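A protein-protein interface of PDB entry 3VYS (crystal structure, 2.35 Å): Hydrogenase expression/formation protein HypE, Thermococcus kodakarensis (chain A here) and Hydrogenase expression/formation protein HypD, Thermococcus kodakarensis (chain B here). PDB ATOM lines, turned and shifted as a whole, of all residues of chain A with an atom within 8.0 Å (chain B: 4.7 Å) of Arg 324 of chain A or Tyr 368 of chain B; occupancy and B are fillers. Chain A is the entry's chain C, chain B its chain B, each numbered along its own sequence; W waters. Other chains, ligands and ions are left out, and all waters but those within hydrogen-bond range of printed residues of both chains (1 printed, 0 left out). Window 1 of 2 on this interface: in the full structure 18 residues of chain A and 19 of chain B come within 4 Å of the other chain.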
ATOM      1  N   SER A 228     -11.765  -9.453 -26.860  1.00  0.00           N
ATOM      2  CA  SER A 228     -11.328 -10.368 -27.903  1.00  0.00           C
ATOM      3  C   SER A 228     -12.456 -10.602 -28.899  1.00  0.00           C
ATOM      4  O   SER A 228     -12.271 -10.450 -30.102  1.00  0.00           O
ATOM      5  CB  SER A 228     -10.872 -11.699 -27.306  1.00  0.00           C
ATOM      6  OG  SER A 228     -11.964 -12.395 -26.753  1.00  0.00           O
ATOM      7  N   ILE A 242      -5.875  -7.886 -37.239  1.00  0.00           N
ATOM      8  CA  ILE A 242      -5.744  -6.935 -36.139  1.00  0.00           C
ATOM      9  C   ILE A 242      -4.630  -7.283 -35.166  1.00  0.00           C
ATOM     10  O   ILE A 242      -4.657  -8.336 -34.521  1.00  0.00           O
ATOM     11  CB  ILE A 242      -7.061  -6.797 -35.357  1.00  0.00           C
ATOM     12  CG1 ILE A 242      -8.106  -6.105 -36.234  1.00  0.00           C
ATOM     13  CG2 ILE A 242      -6.828  -6.027 -34.069  1.00  0.00           C
ATOM     14  CD1 ILE A 242      -9.379  -5.754 -35.500  1.00  0.00           C
ATOM     15  N   LEU A 243      -3.647  -6.392 -35.070  1.00  0.00           N
ATOM     16  CA  LEU A 243      -2.527  -6.589 -34.163  1.00  0.00           C
ATOM     17  C   LEU A 243      -2.764  -5.797 -32.888  1.00  0.00           C
ATOM     18  O   LEU A 243      -2.994  -4.589 -32.928  1.00  0.00           O
ATOM     19  CB  LEU A 243      -1.217  -6.129 -34.805  1.00  0.00           C
ATOM     20  CG  LEU A 243       0.030  -6.347 -33.940  1.00  0.00           C
ATOM     21  CD1 LEU A 243       0.195  -7.835 -33.646  1.00  0.00           C
ATOM     22  CD2 LEU A 243       1.259  -5.797 -34.653  1.00  0.00           C
ATOM     23  N   VAL A 244      -2.713  -6.487 -31.756  1.00  0.00           N
ATOM     24  CA  VAL A 244      -2.920  -5.848 -30.467  1.00  0.00           C
ATOM     25  C   VAL A 244      -1.702  -6.089 -29.585  1.00  0.00           C
ATOM     26  O   VAL A 244      -1.144  -7.185 -29.562  1.00  0.00           O
ATOM     27  CB  VAL A 244      -4.183  -6.404 -29.772  1.00  0.00           C
ATOM     28  CG1 VAL A 244      -4.409  -5.703 -28.453  1.00  0.00           C
ATOM     29  CG2 VAL A 244      -5.379  -6.210 -30.668  1.00  0.00           C
ATOM     30  N   GLU A 246      -0.482  -6.447 -26.000  1.00  0.00           N
ATOM     31  CA  GLU A 246      -0.925  -6.751 -24.643  1.00  0.00           C
ATOM     32  C   GLU A 246      -0.504  -5.731 -23.595  1.00  0.00           C
ATOM     33  O   GLU A 246      -1.228  -5.496 -22.631  1.00  0.00           O
ATOM     34  CB  GLU A 246      -0.413  -8.137 -24.254  1.00  0.00           C
ATOM     35  CG  GLU A 246      -1.147  -8.785 -23.104  1.00  0.00           C
ATOM     36  CD  GLU A 246      -0.868 -10.276 -23.015  1.00  0.00           C
ATOM     37  OE1 GLU A 246       0.309 -10.651 -22.821  1.00  0.00           O
ATOM     38  OE2 GLU A 246      -1.827 -11.071 -23.141  1.00  0.00           O
ATOM     39  N   GLU A 260      -6.823 -13.770 -12.613  1.00  0.00           N
ATOM     40  CA  GLU A 260      -5.857 -14.833 -12.392  1.00  0.00           C
ATOM     41  C   GLU A 260      -6.432 -15.880 -11.458  1.00  0.00           C
ATOM     42  O   GLU A 260      -6.491 -17.056 -11.801  1.00  0.00           O
ATOM     43  CB  GLU A 260      -4.563 -14.268 -11.812  1.00  0.00           C
ATOM     44  CG  GLU A 260      -3.625 -13.729 -12.871  1.00  0.00           C
ATOM     45  CD  GLU A 260      -3.237 -14.798 -13.877  1.00  0.00           C
ATOM     46  OE1 GLU A 260      -2.600 -15.793 -13.468  1.00  0.00           O
ATOM     47  OE2 GLU A 260      -3.575 -14.648 -15.072  1.00  0.00           O
ATOM     48  N   GLY A 263      -8.972 -17.653 -13.015  1.00  0.00           N
ATOM     49  CA  GLY A 263      -8.488 -18.423 -14.147  1.00  0.00           C
ATOM     50  C   GLY A 263      -9.175 -18.066 -15.453  1.00  0.00           C
ATOM     51  O   GLY A 263      -9.386 -18.925 -16.308  1.00  0.00           O
ATOM     52  N   ILE A 264      -9.530 -16.795 -15.609  1.00  0.00           N
ATOM     53  CA  ILE A 264     -10.194 -16.340 -16.825  1.00  0.00           C
ATOM     54  C   ILE A 264      -9.590 -15.038 -17.316  1.00  0.00           C
ATOM     55  O   ILE A 264      -9.309 -14.131 -16.538  1.00  0.00           O
ATOM     56  CB  ILE A 264     -11.708 -16.133 -16.604  1.00  0.00           C
ATOM     57  CG1 ILE A 264     -11.938 -15.240 -15.384  1.00  0.00           C
ATOM     58  CG2 ILE A 264     -12.401 -17.477 -16.444  1.00  0.00           C
ATOM     59  CD1 ILE A 264     -13.398 -14.974 -15.087  1.00  0.00           C
ATOM     60  N   SER A 265      -9.386 -14.957 -18.623  1.00  0.00           N
ATOM     61  CA  SER A 265      -8.816 -13.771 -19.229  1.00  0.00           C
ATOM     62  C   SER A 265      -9.794 -12.609 -19.188  1.00  0.00           C
ATOM     63  O   SER A 265     -10.985 -12.769 -19.473  1.00  0.00           O
ATOM     64  CB  SER A 265      -8.434 -14.053 -20.687  1.00  0.00           C
ATOM     65  OG  SER A 265      -8.097 -12.856 -21.369  1.00  0.00           O
ATOM     66  N   TYR A 267      -9.901 -10.452 -21.190  1.00  0.00           N
ATOM     67  CA  TYR A 267     -10.188 -10.112 -22.577  1.00  0.00           C
ATOM     68  C   TYR A 267     -11.457 -10.795 -23.050  1.00  0.00           C
ATOM     69  O   TYR A 267     -12.093 -10.336 -23.996  1.00  0.00           O
ATOM     70  CB  TYR A 267      -9.065 -10.548 -23.521  1.00  0.00           C
ATOM     71  CG  TYR A 267      -7.686 -10.063 -23.181  1.00  0.00           C
ATOM     72  CD1 TYR A 267      -7.485  -8.833 -22.563  1.00  0.00           C
ATOM     73  CD2 TYR A 267      -6.566 -10.821 -23.529  1.00  0.00           C
ATOM     74  CE1 TYR A 267      -6.200  -8.367 -22.299  1.00  0.00           C
ATOM     75  CE2 TYR A 267      -5.283 -10.365 -23.273  1.00  0.00           C
ATOM     76  CZ  TYR A 267      -5.107  -9.139 -22.659  1.00  0.00           C
ATOM     77  OH  TYR A 267      -3.839  -8.682 -22.404  1.00  0.00           O
ATOM     78  N   ASP A 268     -11.820 -11.895 -22.397  1.00  0.00           N
ATOM     79  CA  ASP A 268     -13.001 -12.659 -22.795  1.00  0.00           C
ATOM     80  C   ASP A 268     -14.274 -12.338 -22.014  1.00  0.00           C
ATOM     81  O   ASP A 268     -15.327 -12.920 -22.275  1.00  0.00           O
ATOM     82  CB  ASP A 268     -12.716 -14.164 -22.684  1.00  0.00           C
ATOM     83  CG  ASP A 268     -11.419 -14.582 -23.380  1.00  0.00           C
ATOM     84  OD1 ASP A 268     -11.154 -14.127 -24.516  1.00  0.00           O
ATOM     85  OD2 ASP A 268     -10.666 -15.384 -22.791  1.00  0.00           O
ATOM     86  N   LYS A 313      -8.403 -12.634 -38.399  1.00  0.00           N
ATOM     87  CA  LYS A 313      -7.908 -13.097 -37.113  1.00  0.00           C
ATOM     88  C   LYS A 313      -7.395 -11.910 -36.305  1.00  0.00           C
ATOM     89  O   LYS A 313      -7.248 -10.804 -36.832  1.00  0.00           O
ATOM     90  CB  LYS A 313      -6.776 -14.105 -37.313  1.00  0.00           C
ATOM     91  CG  LYS A 313      -7.187 -15.366 -38.047  1.00  0.00           C
ATOM     92  CD  LYS A 313      -8.024 -16.272 -37.165  1.00  0.00           C
ATOM     93  CE  LYS A 313      -7.191 -16.865 -36.033  1.00  0.00           C
ATOM     94  NZ  LYS A 313      -8.016 -17.649 -35.062  1.00  0.00           N
ATOM     95  N   VAL A 314      -7.144 -12.147 -35.020  1.00  0.00           N
ATOM     96  CA  VAL A 314      -6.623 -11.123 -34.123  1.00  0.00           C
ATOM     97  C   VAL A 314      -5.300 -11.628 -33.565  1.00  0.00           C
ATOM     98  O   VAL A 314      -5.253 -12.614 -32.828  1.00  0.00           O
ATOM     99  CB  VAL A 314      -7.599 -10.827 -32.962  1.00  0.00           C
ATOM    100  CG1 VAL A 314      -6.905 -10.004 -31.888  1.00  0.00           C
ATOM    101  CG2 VAL A 314      -8.801 -10.065 -33.489  1.00  0.00           C
ATOM    102  N   LEU A 315      -4.226 -10.943 -33.938  1.00  0.00           N
ATOM    103  CA  LEU A 315      -2.885 -11.308 -33.507  1.00  0.00           C
ATOM    104  C   LEU A 315      -2.540 -10.504 -32.262  1.00  0.00           C
ATOM    105  O   LEU A 315      -2.770  -9.293 -32.209  1.00  0.00           O
ATOM    106  CB  LEU A 315      -1.884 -11.011 -34.630  1.00  0.00           C
ATOM    107  CG  LEU A 315      -0.682 -11.948 -34.741  1.00  0.00           C
ATOM    108  CD1 LEU A 315      -1.171 -13.337 -35.114  1.00  0.00           C
ATOM    109  CD2 LEU A 315       0.286 -11.438 -35.793  1.00  0.00           C
ATOM    110  N   LEU A 316      -1.995 -11.181 -31.258  1.00  0.00           N
ATOM    111  CA  LEU A 316      -1.633 -10.530 -30.008  1.00  0.00           C
ATOM    112  C   LEU A 316      -0.136 -10.588 -29.759  1.00  0.00           C
ATOM    113  O   LEU A 316       0.471 -11.660 -29.765  1.00  0.00           O
ATOM    114  CB  LEU A 316      -2.360 -11.197 -28.838  1.00  0.00           C
ATOM    115  CG  LEU A 316      -1.926 -10.796 -27.424  1.00  0.00           C
ATOM    116  CD1 LEU A 316      -2.522  -9.441 -27.062  1.00  0.00           C
ATOM    117  CD2 LEU A 316      -2.384 -11.854 -26.430  1.00  0.00           C
ATOM    118  N   GLU A 317       0.468  -9.429 -29.547  1.00  0.00           N
ATOM    119  CA  GLU A 317       1.885  -9.392 -29.261  1.00  0.00           C
ATOM    120  C   GLU A 317       1.969  -9.342 -27.746  1.00  0.00           C
ATOM    121  O   GLU A 317       1.622  -8.334 -27.133  1.00  0.00           O
ATOM    122  CB  GLU A 317       2.530  -8.148 -29.872  1.00  0.00           C
ATOM    123  CG  GLU A 317       4.032  -8.079 -29.681  1.00  0.00           C
ATOM    124  CD  GLU A 317       4.631  -6.797 -30.227  1.00  0.00           C
ATOM    125  OE1 GLU A 317       5.858  -6.617 -30.091  1.00  0.00           O
ATOM    126  OE2 GLU A 317       3.880  -5.971 -30.789  1.00  0.00           O
ATOM    127  N   THR A 318       2.412 -10.440 -27.144  1.00  0.00           N
ATOM    128  CA  THR A 318       2.525 -10.514 -25.694  1.00  0.00           C
ATOM    129  C   THR A 318       3.504  -9.493 -25.122  1.00  0.00           C
ATOM    130  O   THR A 318       4.298  -8.891 -25.850  1.00  0.00           O
ATOM    131  CB  THR A 318       2.983 -11.906 -25.243  1.00  0.00           C
ATOM    132  OG1 THR A 318       4.328 -12.129 -25.686  1.00  0.00           O
ATOM    133  CG2 THR A 318       2.063 -12.979 -25.818  1.00  0.00           C
ATOM    134  N   GLY A 321       7.086  -9.850 -25.873  1.00  0.00           N
ATOM    135  CA  GLY A 321       7.400  -9.776 -27.287  1.00  0.00           C
ATOM    136  C   GLY A 321       6.937 -10.962 -28.106  1.00  0.00           C
ATOM    137  O   GLY A 321       7.059 -10.952 -29.329  1.00  0.00           O
ATOM    138  N   GLY A 322       6.412 -11.985 -27.437  1.00  0.00           N
ATOM    139  CA  GLY A 322       5.936 -13.159 -28.144  1.00  0.00           C
ATOM    140  C   GLY A 322       4.742 -12.830 -29.019  1.00  0.00           C
ATOM    141  O   GLY A 322       4.250 -11.702 -29.002  1.00  0.00           O
ATOM    142  N   LYS A 323       4.278 -13.812 -29.787  1.00  0.00           N
ATOM    143  CA  LYS A 323       3.136 -13.626 -30.673  1.00  0.00           C
ATOM    144  C   LYS A 323       2.178 -14.808 -30.605  1.00  0.00           C
ATOM    145  O   LYS A 323       2.602 -15.963 -30.636  1.00  0.00           O
ATOM    146  CB  LYS A 323       3.598 -13.472 -32.125  1.00  0.00           C
ATOM    147  CG  LYS A 323       3.376 -12.098 -32.737  1.00  0.00           C
ATOM    148  CD  LYS A 323       4.631 -11.247 -32.674  1.00  0.00           C
ATOM    149  CE  LYS A 323       4.459  -9.953 -33.448  1.00  0.00           C
ATOM    150  NZ  LYS A 323       5.711  -9.149 -33.436  1.00  0.00           N
ATOM    151  N   ARG A 324       0.888 -14.514 -30.510  1.00  0.00           N
ATOM    152  CA  ARG A 324      -0.137 -15.553 -30.479  1.00  0.00           C
ATOM    153  C   ARG A 324      -1.455 -14.925 -30.884  1.00  0.00           C
ATOM    154  O   ARG A 324      -1.571 -13.703 -30.947  1.00  0.00           O
ATOM    155  CB  ARG A 324      -0.266 -16.180 -29.085  1.00  0.00           C
ATOM    156  CG  ARG A 324      -1.009 -15.353 -28.055  1.00  0.00           C
ATOM    157  CD  ARG A 324      -1.126 -16.147 -26.760  1.00  0.00           C
ATOM    158  NE  ARG A 324      -1.721 -15.388 -25.661  1.00  0.00           N
ATOM    159  CZ  ARG A 324      -2.996 -15.025 -25.600  1.00  0.00           C
ATOM    160  NH1 ARG A 324      -3.828 -15.348 -26.580  1.00  0.00           N
ATOM    161  NH2 ARG A 324      -3.442 -14.343 -24.556  1.00  0.00           N
ATOM    162  N   PHE A 325      -2.446 -15.755 -31.173  1.00  0.00           N
ATOM    163  CA  PHE A 325      -3.746 -15.240 -31.563  1.00  0.00           C
ATOM    164  C   PHE A 325      -4.588 -14.955 -30.336  1.00  0.00           C
ATOM    165  O   PHE A 325      -4.425 -15.601 -29.301  1.00  0.00           O
ATOM    166  CB  PHE A 325      -4.495 -16.250 -32.427  1.00  0.00           C
ATOM    167  CG  PHE A 325      -3.935 -16.417 -33.801  1.00  0.00           C
ATOM    168  CD1 PHE A 325      -3.232 -17.567 -34.144  1.00  0.00           C
ATOM    169  CD2 PHE A 325      -4.132 -15.438 -34.764  1.00  0.00           C
ATOM    170  CE1 PHE A 325      -2.736 -17.738 -35.436  1.00  0.00           C
ATOM    171  CE2 PHE A 325      -3.642 -15.597 -36.055  1.00  0.00           C
ATOM    172  CZ  PHE A 325      -2.943 -16.750 -36.392  1.00  0.00           C
ATOM    173  N   MET A 326      -5.474 -13.972 -30.449  1.00  0.00           N
ATOM    174  CA  MET A 326      -6.382 -13.653 -29.359  1.00  0.00           C
ATOM    175  C   MET A 326      -7.672 -14.330 -29.781  1.00  0.00           C
ATOM    176  O   MET A 326      -8.508 -13.737 -30.462  1.00  0.00           O
ATOM    177  CB  MET A 326      -6.606 -12.148 -29.228  1.00  0.00           C
ATOM    178  CG  MET A 326      -7.487 -11.785 -28.046  1.00  0.00           C
ATOM    179  SD  MET A 326      -7.739 -10.015 -27.845  1.00  0.00           S
ATOM    180  CE  MET A 326      -6.290  -9.597 -26.897  1.00  0.00           C
ATOM    181  N   GLU A 327      -7.812 -15.589 -29.389  1.00  0.00           N
ATOM    182  CA  GLU A 327      -8.979 -16.384 -29.745  1.00  0.00           C
ATOM    183  C   GLU A 327     -10.307 -15.894 -29.187  1.00  0.00           C
ATOM    184  O   GLU A 327     -10.417 -15.542 -28.013  1.00  0.00           O
ATOM    185  CB  GLU A 327      -8.765 -17.837 -29.311  1.00  0.00           C
ATOM    186  CG  GLU A 327      -7.773 -18.608 -30.161  1.00  0.00           C
ATOM    187  CD  GLU A 327      -8.228 -18.755 -31.604  1.00  0.00           C
ATOM    188  OE1 GLU A 327      -9.332 -19.296 -31.832  1.00  0.00           O
ATOM    189  OE2 GLU A 327      -7.478 -18.332 -32.512  1.00  0.00           O
ATOM    190  N   ASP B  43       1.212 -23.407 -19.691  1.00  0.00           N
ATOM    191  CA  ASP B  43       0.381 -22.214 -19.732  1.00  0.00           C
ATOM    192  C   ASP B  43       1.279 -20.992 -19.875  1.00  0.00           C
ATOM    193  O   ASP B  43       0.952 -20.061 -20.603  1.00  0.00           O
ATOM    194  CB  ASP B  43      -0.471 -22.110 -18.463  1.00  0.00           C
ATOM    195  CG  ASP B  43      -1.426 -20.933 -18.499  1.00  0.00           C
ATOM    196  OD1 ASP B  43      -1.007 -19.802 -18.171  1.00  0.00           O
ATOM    197  OD2 ASP B  43      -2.597 -21.134 -18.876  1.00  0.00           O
ATOM    198  N   THR B  46       2.744 -21.173 -23.556  1.00  0.00           N
ATOM    199  CA  THR B  46       1.707 -20.853 -24.523  1.00  0.00           C
ATOM    200  C   THR B  46       1.098 -19.464 -24.363  1.00  0.00           C
ATOM    201  O   THR B  46       0.918 -18.753 -25.348  1.00  0.00           O
ATOM    202  CB  THR B  46       0.607 -21.932 -24.486  1.00  0.00           C
ATOM    203  OG1 THR B  46       1.212 -23.208 -24.719  1.00  0.00           O
ATOM    204  CG2 THR B  46      -0.442 -21.693 -25.565  1.00  0.00           C
ATOM    205  N   ARG B  47       0.791 -19.064 -23.134  1.00  0.00           N
ATOM    206  CA  ARG B  47       0.199 -17.749 -22.912  1.00  0.00           C
ATOM    207  C   ARG B  47       1.072 -16.590 -23.414  1.00  0.00           C
ATOM    208  O   ARG B  47       0.569 -15.633 -24.001  1.00  0.00           O
ATOM    209  CB  ARG B  47      -0.093 -17.523 -21.427  1.00  0.00           C
ATOM    210  CG  ARG B  47      -0.798 -16.203 -21.169  1.00  0.00           C
ATOM    211  CD  ARG B  47      -0.771 -15.797 -19.714  1.00  0.00           C
ATOM    212  NE  ARG B  47      -1.382 -16.795 -18.853  1.00  0.00           N
ATOM    213  CZ  ARG B  47      -1.789 -16.552 -17.611  1.00  0.00           C
ATOM    214  NH1 ARG B  47      -1.651 -15.340 -17.094  1.00  0.00           N
ATOM    215  NH2 ARG B  47      -2.327 -17.525 -16.886  1.00  0.00           N
ATOM    216  N   GLN B 363      -6.478 -28.075 -23.686  1.00  0.00           N
ATOM    217  CA  GLN B 363      -7.270 -26.914 -23.326  1.00  0.00           C
ATOM    218  C   GLN B 363      -6.424 -25.651 -23.474  1.00  0.00           C
ATOM    219  O   GLN B 363      -6.876 -24.651 -24.031  1.00  0.00           O
ATOM    220  CB  GLN B 363      -7.792 -27.018 -21.892  1.00  0.00           C
ATOM    221  CG  GLN B 363      -8.547 -25.759 -21.451  1.00  0.00           C
ATOM    222  CD  GLN B 363      -9.305 -25.937 -20.155  1.00  0.00           C
ATOM    223  OE1 GLN B 363      -9.012 -25.287 -19.149  1.00  0.00           O
ATOM    224  NE2 GLN B 363     -10.293 -26.825 -20.172  1.00  0.00           N
ATOM    225  N   ILE B 364      -5.196 -25.703 -22.973  1.00  0.00           N
ATOM    226  CA  ILE B 364      -4.299 -24.567 -23.060  1.00  0.00           C
ATOM    227  C   ILE B 364      -4.060 -24.152 -24.520  1.00  0.00           C
ATOM    228  O   ILE B 364      -4.099 -22.967 -24.846  1.00  0.00           O
ATOM    229  CB  ILE B 364      -2.977 -24.882 -22.343  1.00  0.00           C
ATOM    230  CG1 ILE B 364      -3.253 -25.025 -20.838  1.00  0.00           C
ATOM    231  CG2 ILE B 364      -1.957 -23.772 -22.574  1.00  0.00           C
ATOM    232  CD1 ILE B 364      -2.090 -25.580 -20.044  1.00  0.00           C
ATOM    233  N   PHE B 365      -3.840 -25.119 -25.403  1.00  0.00           N
ATOM    234  CA  PHE B 365      -3.628 -24.796 -26.809  1.00  0.00           C
ATOM    235  C   PHE B 365      -4.879 -24.166 -27.409  1.00  0.00           C
ATOM    236  O   PHE B 365      -4.792 -23.172 -28.126  1.00  0.00           O
ATOM    237  CB  PHE B 365      -3.250 -26.052 -27.602  1.00  0.00           C
ATOM    238  CG  PHE B 365      -1.771 -26.219 -27.801  1.00  0.00           C
ATOM    239  CD1 PHE B 365      -0.895 -26.151 -26.722  1.00  0.00           C
ATOM    240  CD2 PHE B 365      -1.249 -26.450 -29.075  1.00  0.00           C
ATOM    241  CE1 PHE B 365       0.484 -26.312 -26.907  1.00  0.00           C
ATOM    242  CE2 PHE B 365       0.132 -26.615 -29.274  1.00  0.00           C
ATOM    243  CZ  PHE B 365       0.998 -26.544 -28.185  1.00  0.00           C
ATOM    244  N   TYR B 366      -6.041 -24.744 -27.112  1.00  0.00           N
ATOM    245  CA  TYR B 366      -7.306 -24.229 -27.629  1.00  0.00           C
ATOM    246  C   TYR B 366      -7.602 -22.813 -27.137  1.00  0.00           C
ATOM    247  O   TYR B 366      -7.875 -21.895 -27.917  1.00  0.00           O
ATOM    248  CB  TYR B 366      -8.466 -25.124 -27.200  1.00  0.00           C
ATOM    249  CG  TYR B 366      -9.764 -24.717 -27.848  1.00  0.00           C
ATOM    250  CD1 TYR B 366     -10.051 -25.081 -29.163  1.00  0.00           C
ATOM    251  CD2 TYR B 366     -10.673 -23.903 -27.178  1.00  0.00           C
ATOM    252  CE1 TYR B 366     -11.208 -24.638 -29.793  1.00  0.00           C
ATOM    253  CE2 TYR B 366     -11.834 -23.459 -27.801  1.00  0.00           C
ATOM    254  CZ  TYR B 366     -12.094 -23.829 -29.107  1.00  0.00           C
ATOM    255  OH  TYR B 366     -13.242 -23.387 -29.723  1.00  0.00           O
ATOM    256  N   LYS B 367      -7.574 -22.674 -25.819  1.00  0.00           N
ATOM    257  CA  LYS B 367      -7.828 -21.422 -25.134  1.00  0.00           C
ATOM    258  C   LYS B 367      -6.949 -20.275 -25.640  1.00  0.00           C
ATOM    259  O   LYS B 367      -7.392 -19.123 -25.697  1.00  0.00           O
ATOM    260  CB  LYS B 367      -7.612 -21.641 -23.633  1.00  0.00           C
ATOM    261  CG  LYS B 367      -7.665 -20.405 -22.770  1.00  0.00           C
ATOM    262  CD  LYS B 367      -7.491 -20.761 -21.296  1.00  0.00           C
ATOM    263  CE  LYS B 367      -6.166 -21.462 -21.039  1.00  0.00           C
ATOM    264  NZ  LYS B 367      -5.978 -21.817 -19.601  1.00  0.00           N
ATOM    265  N   TYR B 368      -5.706 -20.596 -25.986  1.00  0.00           N
ATOM    266  CA  TYR B 368      -4.743 -19.600 -26.458  1.00  0.00           C
ATOM    267  C   TYR B 368      -4.479 -19.492 -27.966  1.00  0.00           C
ATOM    268  O   TYR B 368      -3.617 -18.728 -28.376  1.00  0.00           O
ATOM    269  CB  TYR B 368      -3.421 -19.728 -25.702  1.00  0.00           C
ATOM    270  CG  TYR B 368      -3.513 -19.316 -24.256  1.00  0.00           C
ATOM    271  CD1 TYR B 368      -3.252 -20.217 -23.243  1.00  0.00           C
ATOM    272  CD2 TYR B 368      -3.867 -18.030 -23.907  1.00  0.00           C
ATOM    273  CE1 TYR B 368      -3.333 -19.847 -21.926  1.00  0.00           C
ATOM    274  CE2 TYR B 368      -3.952 -17.652 -22.592  1.00  0.00           C
ATOM    275  CZ  TYR B 368      -3.686 -18.565 -21.606  1.00  0.00           C
ATOM    276  OH  TYR B 368      -3.769 -18.190 -20.294  1.00  0.00           O
ATOM    277  N   GLY B 369      -5.198 -20.234 -28.798  1.00  0.00           N
ATOM    278  CA  GLY B 369      -4.970 -20.107 -30.225  1.00  0.00           C
ATOM    279  C   GLY B 369      -3.533 -20.248 -30.701  1.00  0.00           C
ATOM    280  O   GLY B 369      -2.968 -19.305 -31.252  1.00  0.00           O
ATOM    281  N   VAL B 370      -2.921 -21.403 -30.471  1.00  0.00           N
ATOM    282  CA  VAL B 370      -1.532 -21.617 -30.873  1.00  0.00           C
ATOM    283  C   VAL B 370      -1.298 -21.471 -32.385  1.00  0.00           C
ATOM    284  O   VAL B 370      -2.139 -21.842 -33.198  1.00  0.00           O
ATOM    285  CB  VAL B 370      -1.035 -22.995 -30.425  1.00  0.00           C
ATOM    286  CG1 VAL B 370      -2.055 -24.063 -30.777  1.00  0.00           C
ATOM    287  CG2 VAL B 370       0.313 -23.294 -31.051  1.00  0.00           C
ATOM    288  N   LEU B 371      -0.144 -20.910 -32.737  1.00  0.00           N
ATOM    289  CA  LEU B 371       0.243 -20.640 -34.115  1.00  0.00           C
ATOM    290  C   LEU B 371       1.688 -21.093 -34.349  1.00  0.00           C
ATOM    291  O   LEU B 371       1.980 -21.614 -35.450  1.00  0.00           O
ATOM    292  CB  LEU B 371       0.047 -19.141 -34.425  1.00  0.00           C
ATOM    293  CG  LEU B 371       1.102 -18.027 -34.536  1.00  0.00           C
ATOM    294  CD1 LEU B 371       0.364 -16.725 -34.253  1.00  0.00           C
ATOM    295  CD2 LEU B 371       2.252 -18.171 -33.550  1.00  0.00           C
HETATM  296  O   HOH W   1      -6.959 -16.183 -26.505  1.00  0.00           O
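The guanidinium group of Arg 47 of chain B lies within salt-bridge range of the side-chain carboxylate of Glu 260 of chain A. NE of Arg 324 of chain A lies within hydrogen-bond range of O of Arg 47 of chain B, 2.8 Å away. O of Tyr 368 of chain B lies close to O of Phe 325 of chain A.
The guanidinium group (NH2) of Arg 47 of chain B is in salt-bridge range of the side-chain carboxylate (OD1) of Asp 43 of chain B (2.9 Å). The side-chain carboxylate (OD2) of Asp 43 of chain B sits close to the side-chain hydroxyl (OH) of Tyr 368 of chain B, at 3.5 Å. The side-chain hydroxyl (OH) of Tyr 368 of chain B is in hydrogen-bond range of the guanidinium group (NE) of Arg 47 of chain B (3.1 Å). NH2 of Arg 324 of chain A lies within salt-bridge range of OE2 of Glu 246 of chain A (3.9 Å). NZ of Lys 313 of chain A lies within salt-bridge range of OE2 of Glu 327 of chain A (2.7 Å). The backbone NH (N) of Leu 316 of chain A sits at hydrogen-bond distance from the backbone carbonyl oxygen (O) of Arg 324 of chain A, at 2.6 Å.
Among the printed residues, pairs that only touch across the chains: Glu 327 of chain A with Gly 369 of chain B (3.2 Å), Phe 325 of chain A with Leu 371 of chain B (3.3 Å), Phe 325 of chain A with Gly 369 of chain B (3.4 Å), Thr 318 of chain A with Arg 47 of chain B (3.5 Å), Arg 324 of chain A with Tyr 368 of chain B (3.6 Å), Arg 324 of chain A with Thr 46 of chain B (3.6 Å), Lys 323 of chain A with Leu 371 of chain B (3.7 Å), Leu 315 of chain A with Leu 371 of chain B (3.8 Å), Glu 327 of chain A with Tyr 366 of chain B (3.98 Å) and Arg 324 of chain A with Leu 371 of chain B (3.98 Å).
Of the printed residues of chain B, Glu 260 of chain A touches Arg 47. Gly 263 of chain A touches none of the printed residues of chain B. Printed residues of chain B within 4 Å of Thr 318 of chain A: Arg 47. Of the printed residues of chain B, Lys 323 of chain A touches Leu 371 (3.7 Å). Of the printed residues of chain B, Arg 324 of chain A touches Thr 46, Arg 47, Tyr 368 and Leu 371. Of the printed residues of chain B, Phe 325 of chain A touches Tyr 368, Gly 369 and Leu 371. Phe 365 of chain B touches none of the printed residues of chain A. Of the printed residues of chain A, Tyr 366 of chain B touches Glu 327 (3.98 Å). Printed residues of chain A within 4 Å of Tyr 368 of chain B: Arg 324 and Phe 325. Gly 369 of chain B touches two residues of chain A. The nearest printed residue of chain A that does not touch Thr 46 of chain B is Thr 318 of chain A (5.9 Å).
Printed residues of chain B that touch a printed residue of chain A: Thr 46, Arg 47, Tyr 366, Tyr 368, Gly 369 and Leu 371. Hydrophobic or aromatic side chains of chain B within 4 Å of the printed part of chain A: Tyr 368 and Leu 371. Of the 24 printed residues of chain A, 7 touch a printed residue of chain B. Among the printed residues, Asp or Glu carboxylates within 4 Å of a Lys or Arg side-chain nitrogen of the other chain: Glu 260 of chain A with Arg 47 of chain B (2.9 Å).
Water W1 lies within hydrogen-bond range of N of Glu 327 of chain A (3.1 Å), O of Lys 367 of chain B (3.1 Å) and NH1 of Arg 324 of chain A (3.2 Å).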
